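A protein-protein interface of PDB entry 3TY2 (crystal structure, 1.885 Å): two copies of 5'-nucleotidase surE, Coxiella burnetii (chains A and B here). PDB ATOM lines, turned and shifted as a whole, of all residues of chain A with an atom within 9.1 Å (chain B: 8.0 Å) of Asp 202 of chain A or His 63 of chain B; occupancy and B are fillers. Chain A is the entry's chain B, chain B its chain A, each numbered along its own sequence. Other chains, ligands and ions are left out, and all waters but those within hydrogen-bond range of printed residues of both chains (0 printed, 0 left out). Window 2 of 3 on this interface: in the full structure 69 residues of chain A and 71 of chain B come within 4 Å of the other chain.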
ATOM      1  N   ARG A 199     -24.676  -5.046 -11.484  1.00  0.00           N
ATOM      2  CA  ARG A 199     -24.393  -5.992 -12.557  1.00  0.00           C
ATOM      3  C   ARG A 199     -25.678  -6.660 -13.007  1.00  0.00           C
ATOM      4  O   ARG A 199     -26.439  -7.163 -12.192  1.00  0.00           O
ATOM      5  CB  ARG A 199     -23.378  -7.049 -12.104  1.00  0.00           C
ATOM      6  CG  ARG A 199     -23.110  -8.147 -13.139  1.00  0.00           C
ATOM      7  CD  ARG A 199     -21.985  -9.072 -12.666  1.00  0.00           C
ATOM      8  NE  ARG A 199     -21.730 -10.184 -13.577  1.00  0.00           N
ATOM      9  CZ  ARG A 199     -22.255 -11.396 -13.443  1.00  0.00           C
ATOM     10  NH1 ARG A 199     -23.078 -11.656 -12.439  1.00  0.00           N
ATOM     11  NH2 ARG A 199     -21.964 -12.349 -14.318  1.00  0.00           N
ATOM     12  N   GLN A 200     -25.926  -6.625 -14.311  1.00  0.00           N
ATOM     13  CA  GLN A 200     -27.072  -7.303 -14.897  1.00  0.00           C
ATOM     14  C   GLN A 200     -26.588  -8.123 -16.082  1.00  0.00           C
ATOM     15  O   GLN A 200     -25.414  -8.074 -16.448  1.00  0.00           O
ATOM     16  CB  GLN A 200     -28.114  -6.290 -15.376  1.00  0.00           C
ATOM     17  CG  GLN A 200     -28.743  -5.451 -14.284  1.00  0.00           C
ATOM     18  CD  GLN A 200     -29.648  -4.359 -14.839  1.00  0.00           C
ATOM     19  OE1 GLN A 200     -29.420  -3.828 -15.934  1.00  0.00           O
ATOM     20  NE2 GLN A 200     -30.684  -4.016 -14.081  1.00  0.00           N
ATOM     21  N   ILE A 201     -27.496  -8.876 -16.686  1.00  0.00           N
ATOM     22  CA  ILE A 201     -27.149  -9.652 -17.864  1.00  0.00           C
ATOM     23  C   ILE A 201     -27.897  -9.097 -19.064  1.00  0.00           C
ATOM     24  O   ILE A 201     -29.120  -8.943 -18.997  1.00  0.00           O
ATOM     25  CB  ILE A 201     -27.524 -11.128 -17.675  1.00  0.00           C
ATOM     26  CG1 ILE A 201     -26.793 -11.702 -16.456  1.00  0.00           C
ATOM     27  CG2 ILE A 201     -27.206 -11.915 -18.937  1.00  0.00           C
ATOM     28  CD1 ILE A 201     -25.291 -11.580 -16.532  1.00  0.00           C
ATOM     29  N   ASP A 202     -27.169  -8.772 -20.138  1.00  0.00           N
ATOM     30  CA  ASP A 202     -27.816  -8.278 -21.358  1.00  0.00           C
ATOM     31  C   ASP A 202     -28.444  -9.431 -22.141  1.00  0.00           C
ATOM     32  O   ASP A 202     -28.133 -10.596 -21.886  1.00  0.00           O
ATOM     33  CB  ASP A 202     -26.882  -7.397 -22.224  1.00  0.00           C
ATOM     34  CG  ASP A 202     -25.852  -8.193 -23.025  1.00  0.00           C
ATOM     35  OD1 ASP A 202     -25.943  -9.440 -23.115  1.00  0.00           O
ATOM     36  OD2 ASP A 202     -24.941  -7.545 -23.589  1.00  0.00           O
ATOM     37  N   PRO A 203     -29.355  -9.110 -23.074  1.00  0.00           N
ATOM     38  CA  PRO A 203     -30.169 -10.108 -23.782  1.00  0.00           C
ATOM     39  C   PRO A 203     -29.370 -11.218 -24.456  1.00  0.00           C
ATOM     40  O   PRO A 203     -29.943 -12.245 -24.814  1.00  0.00           O
ATOM     41  CB  PRO A 203     -30.898  -9.271 -24.832  1.00  0.00           C
ATOM     42  CG  PRO A 203     -31.040  -7.936 -24.186  1.00  0.00           C
ATOM     43  CD  PRO A 203     -29.768  -7.735 -23.407  1.00  0.00           C
ATOM     44  N   ARG A 204     -28.071 -11.024 -24.634  1.00  0.00           N
ATOM     45  CA  ARG A 204     -27.261 -12.053 -25.264  1.00  0.00           C
ATOM     46  C   ARG A 204     -26.391 -12.763 -24.237  1.00  0.00           C
ATOM     47  O   ARG A 204     -25.515 -13.559 -24.591  1.00  0.00           O
ATOM     48  CB  ARG A 204     -26.410 -11.468 -26.391  1.00  0.00           C
ATOM     49  CG  ARG A 204     -26.290 -12.387 -27.602  1.00  0.00           C
ATOM     50  CD  ARG A 204     -26.543 -11.624 -28.893  1.00  0.00           C
ATOM     51  NE  ARG A 204     -25.811 -10.364 -28.909  1.00  0.00           N
ATOM     52  CZ  ARG A 204     -26.326  -9.196 -28.540  1.00  0.00           C
ATOM     53  NH1 ARG A 204     -27.588  -9.122 -28.139  1.00  0.00           N
ATOM     54  NH2 ARG A 204     -25.580  -8.102 -28.576  1.00  0.00           N
ATOM     55  N   GLY A 205     -26.641 -12.468 -22.962  1.00  0.00           N
ATOM     56  CA  GLY A 205     -25.985 -13.163 -21.874  1.00  0.00           C
ATOM     57  C   GLY A 205     -24.618 -12.619 -21.552  1.00  0.00           C
ATOM     58  O   GLY A 205     -23.806 -13.302 -20.928  1.00  0.00           O
ATOM     59  N   HIS A 206     -24.354 -11.388 -21.989  1.00  0.00           N
ATOM     60  CA  HIS A 206     -23.131 -10.705 -21.615  1.00  0.00           C
ATOM     61  C   HIS A 206     -23.434  -9.832 -20.406  1.00  0.00           C
ATOM     62  O   HIS A 206     -24.478  -9.171 -20.353  1.00  0.00           O
ATOM     63  CB  HIS A 206     -22.601  -9.854 -22.771  1.00  0.00           C
ATOM     64  CG  HIS A 206     -22.272 -10.646 -23.997  1.00  0.00           C
ATOM     65  ND1 HIS A 206     -23.008 -10.557 -25.160  1.00  0.00           N
ATOM     66  CD2 HIS A 206     -21.299 -11.555 -24.236  1.00  0.00           C
ATOM     67  CE1 HIS A 206     -22.497 -11.372 -26.066  1.00  0.00           C
ATOM     68  NE2 HIS A 206     -21.459 -11.991 -25.530  1.00  0.00           N
ATOM     69  N   PRO A 207     -22.527  -9.832 -19.423  1.00  0.00           N
ATOM     70  CA  PRO A 207     -22.774  -9.048 -18.216  1.00  0.00           C
ATOM     71  C   PRO A 207     -22.617  -7.572 -18.531  1.00  0.00           C
ATOM     72  O   PRO A 207     -21.805  -7.212 -19.377  1.00  0.00           O
ATOM     73  CB  PRO A 207     -21.663  -9.509 -17.274  1.00  0.00           C
ATOM     74  CG  PRO A 207     -20.538  -9.863 -18.184  1.00  0.00           C
ATOM     75  CD  PRO A 207     -21.189 -10.453 -19.417  1.00  0.00           C
ATOM     76  N   ILE A 208     -23.399  -6.729 -17.871  1.00  0.00           N
ATOM     77  CA  ILE A 208     -23.226  -5.293 -17.998  1.00  0.00           C
ATOM     78  C   ILE A 208     -23.207  -4.708 -16.599  1.00  0.00           C
ATOM     79  O   ILE A 208     -23.777  -5.280 -15.679  1.00  0.00           O
ATOM     80  CB  ILE A 208     -24.357  -4.637 -18.804  1.00  0.00           C
ATOM     81  CG1 ILE A 208     -25.712  -5.072 -18.243  1.00  0.00           C
ATOM     82  CG2 ILE A 208     -24.227  -4.982 -20.284  1.00  0.00           C
ATOM     83  CD1 ILE A 208     -26.901  -4.383 -18.890  1.00  0.00           C
ATOM     84  N   TYR A 209     -22.548  -3.568 -16.451  1.00  0.00           N
ATOM     85  CA  TYR A 209     -22.370  -2.953 -15.156  1.00  0.00           C
ATOM     86  C   TYR A 209     -22.745  -1.479 -15.194  1.00  0.00           C
ATOM     87  O   TYR A 209     -22.179  -0.719 -15.967  1.00  0.00           O
ATOM     88  CB  TYR A 209     -20.900  -3.033 -14.740  1.00  0.00           C
ATOM     89  CG  TYR A 209     -20.371  -4.421 -14.445  1.00  0.00           C
ATOM     90  CD1 TYR A 209     -19.972  -5.274 -15.472  1.00  0.00           C
ATOM     91  CD2 TYR A 209     -20.227  -4.854 -13.135  1.00  0.00           C
ATOM     92  CE1 TYR A 209     -19.463  -6.546 -15.186  1.00  0.00           C
ATOM     93  CE2 TYR A 209     -19.724  -6.109 -12.843  1.00  0.00           C
ATOM     94  CZ  TYR A 209     -19.338  -6.943 -13.866  1.00  0.00           C
ATOM     95  OH  TYR A 209     -18.838  -8.192 -13.548  1.00  0.00           O
ATOM     96  N   TRP A 210     -23.675  -1.078 -14.337  1.00  0.00           N
ATOM     97  CA  TRP A 210     -24.012   0.329 -14.190  1.00  0.00           C
ATOM     98  C   TRP A 210     -23.115   0.960 -13.138  1.00  0.00           C
ATOM     99  O   TRP A 210     -22.817   0.339 -12.108  1.00  0.00           O
ATOM    100  CB  TRP A 210     -25.458   0.494 -13.705  1.00  0.00           C
ATOM    101  CG  TRP A 210     -26.502   0.080 -14.678  1.00  0.00           C
ATOM    102  CD1 TRP A 210     -27.048  -1.163 -14.829  1.00  0.00           C
ATOM    103  CD2 TRP A 210     -27.168   0.930 -15.615  1.00  0.00           C
ATOM    104  NE1 TRP A 210     -27.997  -1.141 -15.826  1.00  0.00           N
ATOM    105  CE2 TRP A 210     -28.091   0.135 -16.319  1.00  0.00           C
ATOM    106  CE3 TRP A 210     -27.063   2.288 -15.930  1.00  0.00           C
ATOM    107  CZ2 TRP A 210     -28.910   0.654 -17.321  1.00  0.00           C
ATOM    108  CZ3 TRP A 210     -27.879   2.801 -16.929  1.00  0.00           C
ATOM    109  CH2 TRP A 210     -28.788   1.986 -17.610  1.00  0.00           C
ATOM    110  N   ALA B  44      -8.813  -1.288 -17.550  1.00  0.00           N
ATOM    111  CA  ALA B  44      -8.457  -0.183 -18.440  1.00  0.00           C
ATOM    112  C   ALA B  44      -9.443  -0.060 -19.604  1.00  0.00           C
ATOM    113  O   ALA B  44     -10.122  -1.026 -19.954  1.00  0.00           O
ATOM    114  CB  ALA B  44      -7.034  -0.397 -18.963  1.00  0.00           C
ATOM    115  N   ASP B  46     -11.074   0.118 -23.328  1.00  0.00           N
ATOM    116  CA  ASP B  46     -10.780  -0.666 -24.524  1.00  0.00           C
ATOM    117  C   ASP B  46     -10.270   0.188 -25.676  1.00  0.00           C
ATOM    118  O   ASP B  46      -9.834  -0.342 -26.698  1.00  0.00           O
ATOM    119  CB  ASP B  46     -11.976  -1.528 -24.962  1.00  0.00           C
ATOM    120  CG  ASP B  46     -13.150  -0.712 -25.502  1.00  0.00           C
ATOM    121  OD1 ASP B  46     -13.339   0.460 -25.105  1.00  0.00           O
ATOM    122  OD2 ASP B  46     -13.913  -1.269 -26.322  1.00  0.00           O
ATOM    123  N   ALA B  60     -25.710   4.855 -19.446  1.00  0.00           N
ATOM    124  CA  ALA B  60     -25.740   3.506 -19.983  1.00  0.00           C
ATOM    125  C   ALA B  60     -24.911   2.579 -19.117  1.00  0.00           C
ATOM    126  O   ALA B  60     -24.022   3.027 -18.392  1.00  0.00           O
ATOM    127  CB  ALA B  60     -25.195   3.502 -21.413  1.00  0.00           C
ATOM    128  N   PRO B  61     -25.202   1.277 -19.184  1.00  0.00           N
ATOM    129  CA  PRO B  61     -24.373   0.301 -18.492  1.00  0.00           C
ATOM    130  C   PRO B  61     -23.138   0.016 -19.346  1.00  0.00           C
ATOM    131  O   PRO B  61     -23.158   0.261 -20.557  1.00  0.00           O
ATOM    132  CB  PRO B  61     -25.279  -0.928 -18.408  1.00  0.00           C
ATOM    133  CG  PRO B  61     -26.150  -0.826 -19.609  1.00  0.00           C
ATOM    134  CD  PRO B  61     -26.342   0.648 -19.884  1.00  0.00           C
ATOM    135  N   LEU B  62     -22.079  -0.487 -18.721  1.00  0.00           N
ATOM    136  CA  LEU B  62     -20.807  -0.700 -19.407  1.00  0.00           C
ATOM    137  C   LEU B  62     -20.491  -2.180 -19.585  1.00  0.00           C
ATOM    138  O   LEU B  62     -20.596  -2.966 -18.634  1.00  0.00           O
ATOM    139  CB  LEU B  62     -19.665  -0.049 -18.623  1.00  0.00           C
ATOM    140  CG  LEU B  62     -19.622   1.472 -18.518  1.00  0.00           C
ATOM    141  CD1 LEU B  62     -20.457   1.971 -17.341  1.00  0.00           C
ATOM    142  CD2 LEU B  62     -18.186   1.903 -18.358  1.00  0.00           C
ATOM    143  N   HIS B  63     -20.085  -2.558 -20.793  1.00  0.00           N
ATOM    144  CA  HIS B  63     -19.621  -3.920 -21.030  1.00  0.00           C
ATOM    145  C   HIS B  63     -18.168  -4.037 -20.620  1.00  0.00           C
ATOM    146  O   HIS B  63     -17.361  -3.151 -20.901  1.00  0.00           O
ATOM    147  CB  HIS B  63     -19.784  -4.324 -22.492  1.00  0.00           C
ATOM    148  CG  HIS B  63     -21.209  -4.528 -22.902  1.00  0.00           C
ATOM    149  ND1 HIS B  63     -22.043  -3.484 -23.238  1.00  0.00           N
ATOM    150  CD2 HIS B  63     -21.949  -5.653 -23.014  1.00  0.00           C
ATOM    151  CE1 HIS B  63     -23.235  -3.962 -23.548  1.00  0.00           C
ATOM    152  NE2 HIS B  63     -23.201  -5.276 -23.422  1.00  0.00           N
ATOM    153  N   ILE B  64     -17.842  -5.146 -19.964  1.00  0.00           N
ATOM    154  CA  ILE B  64     -16.497  -5.397 -19.471  1.00  0.00           C
ATOM    155  C   ILE B  64     -16.095  -6.806 -19.882  1.00  0.00           C
ATOM    156  O   ILE B  64     -16.921  -7.715 -19.847  1.00  0.00           O
ATOM    157  CB  ILE B  64     -16.472  -5.269 -17.940  1.00  0.00           C
ATOM    158  CG1 ILE B  64     -16.983  -3.880 -17.524  1.00  0.00           C
ATOM    159  CG2 ILE B  64     -15.084  -5.523 -17.405  1.00  0.00           C
ATOM    160  CD1 ILE B  64     -16.817  -3.581 -16.034  1.00  0.00           C
ATOM    161  N   LYS B  65     -14.839  -6.989 -20.283  1.00  0.00           N
ATOM    162  CA  LYS B  65     -14.369  -8.305 -20.734  1.00  0.00           C
ATOM    163  C   LYS B  65     -12.986  -8.624 -20.184  1.00  0.00           C
ATOM    164  O   LYS B  65     -12.200  -7.717 -19.909  1.00  0.00           O
ATOM    165  CB  LYS B  65     -14.357  -8.376 -22.268  1.00  0.00           C
ATOM    166  CG  LYS B  65     -13.299  -7.500 -22.933  1.00  0.00           C
ATOM    167  CD  LYS B  65     -13.746  -6.999 -24.304  1.00  0.00           C
ATOM    168  CE  LYS B  65     -14.796  -5.894 -24.185  1.00  0.00           C
ATOM    169  NZ  LYS B  65     -15.244  -5.388 -25.518  1.00  0.00           N
ATOM    170  N   ILE B  72      -8.382  -6.564 -17.640  1.00  0.00           N
ATOM    171  CA  ILE B  72      -9.821  -6.365 -17.782  1.00  0.00           C
ATOM    172  C   ILE B  72     -10.065  -5.132 -18.648  1.00  0.00           C
ATOM    173  O   ILE B  72      -9.558  -4.052 -18.354  1.00  0.00           O
ATOM    174  CB  ILE B  72     -10.503  -6.166 -16.416  1.00  0.00           C
ATOM    175  CG1 ILE B  72     -10.373  -7.428 -15.566  1.00  0.00           C
ATOM    176  CG2 ILE B  72     -11.968  -5.783 -16.608  1.00  0.00           C
ATOM    177  CD1 ILE B  72     -10.774  -7.236 -14.094  1.00  0.00           C
ATOM    178  N   SER B  73     -10.842  -5.293 -19.714  1.00  0.00           N
ATOM    179  CA  SER B  73     -11.050  -4.220 -20.677  1.00  0.00           C
ATOM    180  C   SER B  73     -12.479  -3.692 -20.554  1.00  0.00           C
ATOM    181  O   SER B  73     -13.437  -4.466 -20.575  1.00  0.00           O
ATOM    182  CB  SER B  73     -10.766  -4.749 -22.089  1.00  0.00           C
ATOM    183  OG  SER B  73     -11.066  -3.794 -23.089  1.00  0.00           O
ATOM    184  N   VAL B  74     -12.619  -2.377 -20.401  1.00  0.00           N
ATOM    185  CA  VAL B  74     -13.912  -1.771 -20.126  1.00  0.00           C
ATOM    186  C   VAL B  74     -14.307  -0.851 -21.275  1.00  0.00           C
ATOM    187  O   VAL B  74     -13.487  -0.040 -21.735  1.00  0.00           O
ATOM    188  CB  VAL B  74     -13.861  -0.929 -18.833  1.00  0.00           C
ATOM    189  CG1 VAL B  74     -15.203  -0.265 -18.583  1.00  0.00           C
ATOM    190  CG2 VAL B  74     -13.454  -1.800 -17.632  1.00  0.00           C
ATOM    191  N   GLU B  75     -15.549  -0.971 -21.742  1.00  0.00           N
ATOM    192  CA  GLU B  75     -16.008  -0.125 -22.838  1.00  0.00           C
ATOM    193  C   GLU B  75     -16.490   1.212 -22.290  1.00  0.00           C
ATOM    194  O   GLU B  75     -17.666   1.565 -22.395  1.00  0.00           O
ATOM    195  CB  GLU B  75     -17.107  -0.819 -23.655  1.00  0.00           C
ATOM    196  CG  GLU B  75     -16.617  -2.092 -24.340  1.00  0.00           C
ATOM    197  CD  GLU B  75     -17.727  -2.827 -25.091  1.00  0.00           C
ATOM    198  OE1 GLU B  75     -18.847  -2.286 -25.211  1.00  0.00           O
ATOM    199  OE2 GLU B  75     -17.469  -3.955 -25.544  1.00  0.00           O
ATOM    200  N   GLY B  76     -15.571   1.947 -21.678  1.00  0.00           N
ATOM    201  CA  GLY B  76     -15.912   3.207 -21.042  1.00  0.00           C
ATOM    202  C   GLY B  76     -14.670   4.003 -20.727  1.00  0.00           C
ATOM    203  O   GLY B  76     -13.622   3.765 -21.327  1.00  0.00           O
ATOM    204  N   LEU B  84     -15.711   1.545 -11.163  1.00  0.00           N
ATOM    205  CA  LEU B  84     -16.316   0.207 -11.157  1.00  0.00           C
ATOM    206  C   LEU B  84     -15.437  -0.805 -10.421  1.00  0.00           C
ATOM    207  O   LEU B  84     -15.938  -1.626  -9.645  1.00  0.00           O
ATOM    208  CB  LEU B  84     -16.593  -0.278 -12.583  1.00  0.00           C
ATOM    209  CG  LEU B  84     -17.563   0.618 -13.356  1.00  0.00           C
ATOM    210  CD1 LEU B  84     -17.763   0.096 -14.777  1.00  0.00           C
ATOM    211  CD2 LEU B  84     -18.886   0.734 -12.617  1.00  0.00           C
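A ring nitrogen (NE2) of His 63 of chain B is in hydrogen-bond range of the side-chain carboxylate (OD2) of Asp 202 of chain A (2.9 Å). The backbone NH (N) of Leu 62 of chain B lies within hydrogen-bond range of the backbone carbonyl oxygen (O) of Tyr 209 of chain A, 2.8 Å away.
OE1 of Gln 200 of chain A lies within hydrogen-bond range of NE1 of Trp 210 of chain A (3.0 Å). O of Gln 200 of chain A lies within hydrogen-bond range of N of Ile 208 of chain A. OD1 of Asp 202 of chain A sits at hydrogen-bond distance from N of His 206 of chain A. O of His 63 of chain B lies within hydrogen-bond range of N of Glu 75 of chain B. N of Arg 204 of chain A lies close to OD1 of Asp 202 of chain A (3.1 Å). OD1 of Asp 202 of chain A lies within hydrogen-bond range of N of Gly 205 of chain A (3.1 Å).
No position is printed for both chains. Of the 11 pairs that touch across the chains among the printed residues, none has its exchanged pair printed and touching as well.
Among the printed residues, merely in contact across the chains: Pro 207 of chain A with His 63 of chain B (3.96 Å), Ile 208 of chain A with Pro 61 of chain B (3.7 Å), Ile 208 of chain A with Leu 62 of chain B (3.6 Å), Ile 208 of chain A with His 63 of chain B (3.3 Å), Tyr 209 of chain A with Pro 61 of chain B (3.5 Å), Tyr 209 of chain A with Ile 64 of chain B (3.6 Å), Trp 210 of chain A with Ala 60 of chain B (3.7 Å), Trp 210 of chain A with Pro 61 of chain B (3.6 Å) and Trp 210 of chain A with Leu 84 of chain B (3.98 Å).
No residue of chain B comes within 4 Å of Pro 203 of chain A. Printed residues of chain B within 4 Å of Ile 208 of chain A: Pro 61 (3.7 Å), Leu 62 (3.6 Å) and His 63 (3.3 Å). Printed residues of chain B within 4 Å of Tyr 209 of chain A: Pro 61 (3.5 Å), Leu 62 (2.8 Å) and Ile 64 (3.6 Å). Of the printed residues of chain B, Trp 210 of chain A touches Ala 60 (3.7 Å), Pro 61 (3.6 Å) and Leu 84 (3.98 Å). Of the printed residues of chain A, Pro 61 of chain B touches Ile 208 (3.7 Å), Tyr 209 (3.5 Å) and Trp 210 (3.6 Å). Of the printed residues of chain A, Leu 62 of chain B touches Ile 208 (3.6 Å) and Tyr 209 (2.8 Å). His 63 of chain B touches just these residues of chain A: Asp 202 (2.9 Å), Pro 207 (3.96 Å) and Ile 208 (3.3 Å). Of the printed residues of chain A, Ile 64 of chain B touches Tyr 209. The nearest residue of chain B that does not touch Asp 202 of chain A is Pro 61 of chain B (7.1 Å).
Printed residues of chain B that touch a printed residue of chain A: Ala 60, Pro 61, Leu 62, His 63, Ile 64 and Leu 84. Of the 12 printed residues of chain A, 5 touch a printed residue of chain B. Printed residues of chain A that touch a printed residue of chain B: Asp 202, Pro 207, Ile 208, Tyr 209 and Trp 210. Among the printed residues, no Asp or Glu carboxylate lies within 4 Å of a Lys or Arg side-chain nitrogen of the other chain.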
